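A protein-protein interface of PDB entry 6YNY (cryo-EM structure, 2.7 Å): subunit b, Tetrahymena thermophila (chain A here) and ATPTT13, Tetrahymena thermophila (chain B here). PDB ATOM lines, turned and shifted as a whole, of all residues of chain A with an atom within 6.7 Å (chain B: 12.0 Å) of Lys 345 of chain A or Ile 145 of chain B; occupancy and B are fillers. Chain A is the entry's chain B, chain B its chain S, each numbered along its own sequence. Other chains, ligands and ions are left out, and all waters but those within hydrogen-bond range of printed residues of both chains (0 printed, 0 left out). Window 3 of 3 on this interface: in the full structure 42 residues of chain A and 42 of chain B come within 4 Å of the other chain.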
ATOM      1  N   ARG A 240     -33.643 -15.754  -5.500  1.00  0.00           N
ATOM      2  CA  ARG A 240     -33.088 -15.888  -6.841  1.00  0.00           C
ATOM      3  C   ARG A 240     -34.198 -16.034  -7.874  1.00  0.00           C
ATOM      4  O   ARG A 240     -34.176 -15.382  -8.924  1.00  0.00           O
ATOM      5  CB  ARG A 240     -32.138 -17.085  -6.892  1.00  0.00           C
ATOM      6  CG  ARG A 240     -31.499 -17.317  -8.249  1.00  0.00           C
ATOM      7  CD  ARG A 240     -30.759 -18.641  -8.293  1.00  0.00           C
ATOM      8  NE  ARG A 240     -29.518 -18.604  -7.524  1.00  0.00           N
ATOM      9  CZ  ARG A 240     -28.673 -19.624  -7.416  1.00  0.00           C
ATOM     10  NH1 ARG A 240     -28.930 -20.774  -8.025  1.00  0.00           N
ATOM     11  NH2 ARG A 240     -27.566 -19.496  -6.697  1.00  0.00           N
ATOM     12  N   ALA A 241     -35.181 -16.892  -7.592  1.00  0.00           N
ATOM     13  CA  ALA A 241     -36.276 -17.098  -8.533  1.00  0.00           C
ATOM     14  C   ALA A 241     -37.112 -15.839  -8.708  1.00  0.00           C
ATOM     15  O   ALA A 241     -37.726 -15.646  -9.763  1.00  0.00           O
ATOM     16  CB  ALA A 241     -37.159 -18.254  -8.066  1.00  0.00           C
ATOM     17  N   ILE A 244     -34.697 -13.059 -10.784  1.00  0.00           N
ATOM     18  CA  ILE A 244     -34.620 -13.413 -12.198  1.00  0.00           C
ATOM     19  C   ILE A 244     -35.930 -13.077 -12.897  1.00  0.00           C
ATOM     20  O   ILE A 244     -35.941 -12.638 -14.054  1.00  0.00           O
ATOM     21  CB  ILE A 244     -34.256 -14.900 -12.359  1.00  0.00           C
ATOM     22  CG1 ILE A 244     -34.070 -15.239 -13.837  1.00  0.00           C
ATOM     23  CG2 ILE A 244     -35.336 -15.784 -11.759  1.00  0.00           C
ATOM     24  CD1 ILE A 244     -33.556 -16.638 -14.085  1.00  0.00           C
ATOM     25  N   GLN A 340     -28.977 -10.856 -24.232  1.00  0.00           N
ATOM     26  CA  GLN A 340     -29.858 -10.331 -23.194  1.00  0.00           C
ATOM     27  C   GLN A 340     -30.208 -11.413 -22.181  1.00  0.00           C
ATOM     28  O   GLN A 340     -30.144 -11.189 -20.967  1.00  0.00           O
ATOM     29  CB  GLN A 340     -31.122  -9.749 -23.826  1.00  0.00           C
ATOM     30  CG  GLN A 340     -31.976  -8.932 -22.871  1.00  0.00           C
ATOM     31  CD  GLN A 340     -33.047  -8.135 -23.589  1.00  0.00           C
ATOM     32  OE1 GLN A 340     -33.592  -8.576 -24.600  1.00  0.00           O
ATOM     33  NE2 GLN A 340     -33.348  -6.950 -23.074  1.00  0.00           N
ATOM     34  N   LEU A 341     -30.585 -12.599 -22.665  1.00  0.00           N
ATOM     35  CA  LEU A 341     -30.827 -13.720 -21.765  1.00  0.00           C
ATOM     36  C   LEU A 341     -29.527 -14.247 -21.173  1.00  0.00           C
ATOM     37  O   LEU A 341     -29.521 -14.761 -20.048  1.00  0.00           O
ATOM     38  CB  LEU A 341     -31.566 -14.834 -22.507  1.00  0.00           C
ATOM     39  CG  LEU A 341     -31.903 -16.083 -21.690  1.00  0.00           C
ATOM     40  CD1 LEU A 341     -32.836 -15.734 -20.541  1.00  0.00           C
ATOM     41  CD2 LEU A 341     -32.521 -17.148 -22.580  1.00  0.00           C
ATOM     42  N   LYS A 342     -28.421 -14.132 -21.912  1.00  0.00           N
ATOM     43  CA  LYS A 342     -27.132 -14.578 -21.396  1.00  0.00           C
ATOM     44  C   LYS A 342     -26.775 -13.848 -20.107  1.00  0.00           C
ATOM     45  O   LYS A 342     -26.296 -14.462 -19.147  1.00  0.00           O
ATOM     46  CB  LYS A 342     -26.047 -14.365 -22.451  1.00  0.00           C
ATOM     47  CG  LYS A 342     -24.678 -14.905 -22.062  1.00  0.00           C
ATOM     48  CD  LYS A 342     -23.603 -14.472 -23.049  1.00  0.00           C
ATOM     49  CE  LYS A 342     -23.853 -15.031 -24.442  1.00  0.00           C
ATOM     50  NZ  LYS A 342     -22.775 -14.653 -25.397  1.00  0.00           N
ATOM     51  N   SER A 343     -27.002 -12.533 -20.069  1.00  0.00           N
ATOM     52  CA  SER A 343     -26.694 -11.766 -18.865  1.00  0.00           C
ATOM     53  C   SER A 343     -27.492 -12.276 -17.673  1.00  0.00           C
ATOM     54  O   SER A 343     -26.992 -12.293 -16.543  1.00  0.00           O
ATOM     55  CB  SER A 343     -26.977 -10.284 -19.105  1.00  0.00           C
ATOM     56  OG  SER A 343     -28.341 -10.071 -19.427  1.00  0.00           O
ATOM     57  N   ILE A 344     -28.736 -12.699 -17.907  1.00  0.00           N
ATOM     58  CA  ILE A 344     -29.552 -13.235 -16.822  1.00  0.00           C
ATOM     59  C   ILE A 344     -28.941 -14.524 -16.288  1.00  0.00           C
ATOM     60  O   ILE A 344     -28.891 -14.750 -15.073  1.00  0.00           O
ATOM     61  CB  ILE A 344     -30.997 -13.459 -17.304  1.00  0.00           C
ATOM     62  CG1 ILE A 344     -31.599 -12.157 -17.841  1.00  0.00           C
ATOM     63  CG2 ILE A 344     -31.848 -14.019 -16.180  1.00  0.00           C
ATOM     64  CD1 ILE A 344     -31.612 -11.023 -16.840  1.00  0.00           C
ATOM     65  N   LYS A 345     -28.466 -15.387 -17.186  1.00  0.00           N
ATOM     66  CA  LYS A 345     -27.889 -16.657 -16.759  1.00  0.00           C
ATOM     67  C   LYS A 345     -26.610 -16.441 -15.960  1.00  0.00           C
ATOM     68  O   LYS A 345     -26.350 -17.161 -14.988  1.00  0.00           O
ATOM     69  CB  LYS A 345     -27.619 -17.543 -17.974  1.00  0.00           C
ATOM     70  CG  LYS A 345     -27.250 -18.977 -17.619  1.00  0.00           C
ATOM     71  CD  LYS A 345     -27.026 -19.838 -18.857  1.00  0.00           C
ATOM     72  CE  LYS A 345     -28.275 -19.936 -19.724  1.00  0.00           C
ATOM     73  NZ  LYS A 345     -29.475 -20.353 -18.946  1.00  0.00           N
ATOM     74  N   GLU A 346     -25.799 -15.456 -16.351  1.00  0.00           N
ATOM     75  CA  GLU A 346     -24.567 -15.179 -15.619  1.00  0.00           C
ATOM     76  C   GLU A 346     -24.861 -14.713 -14.198  1.00  0.00           C
ATOM     77  O   GLU A 346     -24.131 -15.060 -13.262  1.00  0.00           O
ATOM     78  CB  GLU A 346     -23.741 -14.131 -16.364  1.00  0.00           C
ATOM     79  CG  GLU A 346     -23.255 -14.584 -17.729  1.00  0.00           C
ATOM     80  CD  GLU A 346     -22.462 -13.511 -18.450  1.00  0.00           C
ATOM     81  OE1 GLU A 346     -22.289 -12.415 -17.879  1.00  0.00           O
ATOM     82  OE2 GLU A 346     -22.013 -13.766 -19.587  1.00  0.00           O
ATOM     83  N   ASN A 347     -25.924 -13.928 -14.015  1.00  0.00           N
ATOM     84  CA  ASN A 347     -26.293 -13.505 -12.668  1.00  0.00           C
ATOM     85  C   ASN A 347     -26.647 -14.702 -11.797  1.00  0.00           C
ATOM     86  O   ASN A 347     -26.269 -14.757 -10.620  1.00  0.00           O
ATOM     87  CB  ASN A 347     -27.465 -12.525 -12.728  1.00  0.00           C
ATOM     88  CG  ASN A 347     -27.105 -11.226 -13.421  1.00  0.00           C
ATOM     89  OD1 ASN A 347     -26.547 -10.316 -12.809  1.00  0.00           O
ATOM     90  ND2 ASN A 347     -27.429 -11.133 -14.705  1.00  0.00           N
ATOM     91  N   ASP A 348     -27.373 -15.673 -12.355  1.00  0.00           N
ATOM     92  CA  ASP A 348     -27.694 -16.881 -11.603  1.00  0.00           C
ATOM     93  C   ASP A 348     -26.425 -17.621 -11.198  1.00  0.00           C
ATOM     94  O   ASP A 348     -26.285 -18.059 -10.050  1.00  0.00           O
ATOM     95  CB  ASP A 348     -28.607 -17.783 -12.434  1.00  0.00           C
ATOM     96  CG  ASP A 348     -29.046 -19.025 -11.684  1.00  0.00           C
ATOM     97  OD1 ASP A 348     -28.627 -19.207 -10.522  1.00  0.00           O
ATOM     98  OD2 ASP A 348     -29.818 -19.823 -12.256  1.00  0.00           O
ATOM     99  N   VAL A 349     -25.484 -17.770 -12.132  1.00  0.00           N
ATOM    100  CA  VAL A 349     -24.217 -18.415 -11.807  1.00  0.00           C
ATOM    101  C   VAL A 349     -23.438 -17.582 -10.800  1.00  0.00           C
ATOM    102  O   VAL A 349     -22.870 -18.114  -9.838  1.00  0.00           O
ATOM    103  CB  VAL A 349     -23.401 -18.659 -13.089  1.00  0.00           C
ATOM    104  CG1 VAL A 349     -22.040 -19.245 -12.750  1.00  0.00           C
ATOM    105  CG2 VAL A 349     -24.161 -19.577 -14.031  1.00  0.00           C
ATOM    106  N   ARG A 350     -23.399 -16.262 -10.999  1.00  0.00           N
ATOM    107  CA  ARG A 350     -22.701 -15.395 -10.055  1.00  0.00           C
ATOM    108  C   ARG A 350     -23.314 -15.497  -8.665  1.00  0.00           C
ATOM    109  O   ARG A 350     -22.593 -15.502  -7.659  1.00  0.00           O
ATOM    110  CB  ARG A 350     -22.733 -13.952 -10.556  1.00  0.00           C
ATOM    111  CG  ARG A 350     -22.031 -12.958  -9.647  1.00  0.00           C
ATOM    112  CD  ARG A 350     -22.096 -11.552 -10.218  1.00  0.00           C
ATOM    113  NE  ARG A 350     -21.386 -11.448 -11.490  1.00  0.00           N
ATOM    114  CZ  ARG A 350     -20.080 -11.227 -11.611  1.00  0.00           C
ATOM    115  NH1 ARG A 350     -19.532 -11.150 -12.815  1.00  0.00           N
ATOM    116  NH2 ARG A 350     -19.319 -11.086 -10.533  1.00  0.00           N
ATOM    117  N   ILE B 138     -26.896 -29.852  -3.115  1.00  0.00           N
ATOM    118  CA  ILE B 138     -28.255 -29.445  -3.464  1.00  0.00           C
ATOM    119  C   ILE B 138     -28.232 -28.411  -4.582  1.00  0.00           C
ATOM    120  O   ILE B 138     -29.052 -28.457  -5.507  1.00  0.00           O
ATOM    121  CB  ILE B 138     -28.991 -28.916  -2.220  1.00  0.00           C
ATOM    122  CG1 ILE B 138     -29.115 -30.022  -1.170  1.00  0.00           C
ATOM    123  CG2 ILE B 138     -30.365 -28.383  -2.606  1.00  0.00           C
ATOM    124  CD1 ILE B 138     -29.664 -29.552   0.158  1.00  0.00           C
ATOM    125  N   LEU B 139     -27.295 -27.463  -4.518  1.00  0.00           N
ATOM    126  CA  LEU B 139     -27.254 -26.399  -5.515  1.00  0.00           C
ATOM    127  C   LEU B 139     -26.593 -26.863  -6.808  1.00  0.00           C
ATOM    128  O   LEU B 139     -27.000 -26.446  -7.896  1.00  0.00           O
ATOM    129  CB  LEU B 139     -26.522 -25.184  -4.946  1.00  0.00           C
ATOM    130  CG  LEU B 139     -27.204 -24.529  -3.742  1.00  0.00           C
ATOM    131  CD1 LEU B 139     -26.335 -23.425  -3.165  1.00  0.00           C
ATOM    132  CD2 LEU B 139     -28.572 -23.985  -4.128  1.00  0.00           C
ATOM    133  N   SER B 140     -25.576 -27.721  -6.713  1.00  0.00           N
ATOM    134  CA  SER B 140     -24.971 -28.282  -7.914  1.00  0.00           C
ATOM    135  C   SER B 140     -25.881 -29.288  -8.605  1.00  0.00           C
ATOM    136  O   SER B 140     -25.559 -29.727  -9.715  1.00  0.00           O
ATOM    137  CB  SER B 140     -23.637 -28.946  -7.572  1.00  0.00           C
ATOM    138  OG  SER B 140     -22.741 -28.017  -6.991  1.00  0.00           O
ATOM    139  N   LYS B 141     -26.996 -29.662  -7.977  1.00  0.00           N
ATOM    140  CA  LYS B 141     -27.929 -30.596  -8.598  1.00  0.00           C
ATOM    141  C   LYS B 141     -28.440 -30.053  -9.926  1.00  0.00           C
ATOM    142  O   LYS B 141     -28.235 -30.658 -10.984  1.00  0.00           O
ATOM    143  CB  LYS B 141     -29.092 -30.871  -7.641  1.00  0.00           C
ATOM    144  CG  LYS B 141     -30.138 -31.846  -8.170  1.00  0.00           C
ATOM    145  CD  LYS B 141     -29.542 -33.205  -8.521  1.00  0.00           C
ATOM    146  CE  LYS B 141     -28.848 -33.851  -7.330  1.00  0.00           C
ATOM    147  NZ  LYS B 141     -29.733 -33.933  -6.134  1.00  0.00           N
ATOM    148  N   GLY B 142     -29.113 -28.904  -9.886  1.00  0.00           N
ATOM    149  CA  GLY B 142     -29.629 -28.288 -11.088  1.00  0.00           C
ATOM    150  C   GLY B 142     -29.495 -26.781 -11.024  1.00  0.00           C
ATOM    151  O   GLY B 142     -29.329 -26.192  -9.953  1.00  0.00           O
ATOM    152  N   ASP B 143     -29.568 -26.163 -12.198  1.00  0.00           N
ATOM    153  CA  ASP B 143     -29.465 -24.718 -12.335  1.00  0.00           C
ATOM    154  C   ASP B 143     -30.862 -24.132 -12.481  1.00  0.00           C
ATOM    155  O   ASP B 143     -31.636 -24.567 -13.341  1.00  0.00           O
ATOM    156  CB  ASP B 143     -28.600 -24.344 -13.539  1.00  0.00           C
ATOM    157  CG  ASP B 143     -28.267 -22.866 -13.580  1.00  0.00           C
ATOM    158  OD1 ASP B 143     -28.668 -22.139 -12.649  1.00  0.00           O
ATOM    159  OD2 ASP B 143     -27.603 -22.431 -14.546  1.00  0.00           O
ATOM    160  N   LEU B 144     -31.181 -23.148 -11.639  1.00  0.00           N
ATOM    161  CA  LEU B 144     -32.517 -22.562 -11.646  1.00  0.00           C
ATOM    162  C   LEU B 144     -32.857 -21.986 -13.016  1.00  0.00           C
ATOM    163  O   LEU B 144     -33.789 -22.451 -13.684  1.00  0.00           O
ATOM    164  CB  LEU B 144     -32.614 -21.482 -10.568  1.00  0.00           C
ATOM    165  CG  LEU B 144     -33.994 -20.851 -10.374  1.00  0.00           C
ATOM    166  CD1 LEU B 144     -35.003 -21.887  -9.895  1.00  0.00           C
ATOM    167  CD2 LEU B 144     -33.912 -19.687  -9.403  1.00  0.00           C
ATOM    168  N   ILE B 145     -32.093 -20.987 -13.456  1.00  0.00           N
ATOM    169  CA  ILE B 145     -32.343 -20.262 -14.707  1.00  0.00           C
ATOM    170  C   ILE B 145     -33.830 -20.182 -15.035  1.00  0.00           C
ATOM    171  O   ILE B 145     -34.658 -19.954 -14.153  1.00  0.00           O
ATOM    172  CB  ILE B 145     -31.557 -20.889 -15.891  1.00  0.00           C
ATOM    173  CG1 ILE B 145     -31.871 -22.380 -16.072  1.00  0.00           C
ATOM    174  CG2 ILE B 145     -30.063 -20.682 -15.695  1.00  0.00           C
ATOM    175  CD1 ILE B 145     -33.209 -22.670 -16.732  1.00  0.00           C
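The guanidinium group of Arg 240 of chain A lies within salt-bridge range of the side-chain carboxylate of Asp 348 of chain A (3.0 Å).
Of the 8 printed residues of chain B, 3 touch a printed residue of chain A. Among the printed residues, 7 pairs touch across the chains.
Arg 240 of chain A touches Leu 144 of chain B. N of Ala 241 of chain A touches CD2 of Leu 144 of chain B (3.6 Å). Ile 244 of chain A touches Ile 145 of chain B (CD1 to O, 3.5 Å). Lys 345 of chain A touches Ile 145 of chain B (NZ to CG2, 3.3 Å). Asp 348 of chain A touches Leu 144 of chain B.
The backbone NH of Ile 145 of chain B lies within hydrogen-bond range of the side-chain carboxylate of Asp 348 of chain A. OD1 of Asp 143 of chain B sits close to OD2 of Asp 348 of chain A.
Printed residues of chain B within 4 Å of Arg 240 of chain A: Leu 144 (3.5 Å). Ala 241 of chain A touches just one residue of chain B: Leu 144. Ile 244 of chain A touches just one residue of chain B: Ile 145 (3.5 Å). No residue of chain B comes within 4 Å of Leu 341 of chain A. Ser 343 of chain A touches none of the printed residues of chain B. No residue of chain B comes within 4 Å of Ile 344 of chain A. Of the printed residues of chain B, Lys 345 of chain A touches Ile 145 (3.3 Å). No residue of chain B comes within 4 Å of Glu 346 of chain A. Asn 347 of chain A touches none of the printed residues of chain B. Of chain B, only Asp 143 (2.6 Å), Leu 144 (3.6 Å) and Ile 145 (2.8 Å) come within 4 Å of Asp 348 of chain A. No residue of chain B comes within 4 Å of Val 349 of chain A. Gly 142 of chain B touches none of the printed residues of chain A. Of the printed residues of chain A, Leu 144 of chain B touches Arg 240, Ala 241 and Asp 348. Ile 145 of chain B touches just these residues of chain A: Ile 244 (3.5 Å), Lys 345 (3.3 Å) and Asp 348 (2.8 Å). The nearest residue of chain B that does not touch Lys 345 of chain A is Asp 143 of chain B (4.6 Å).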
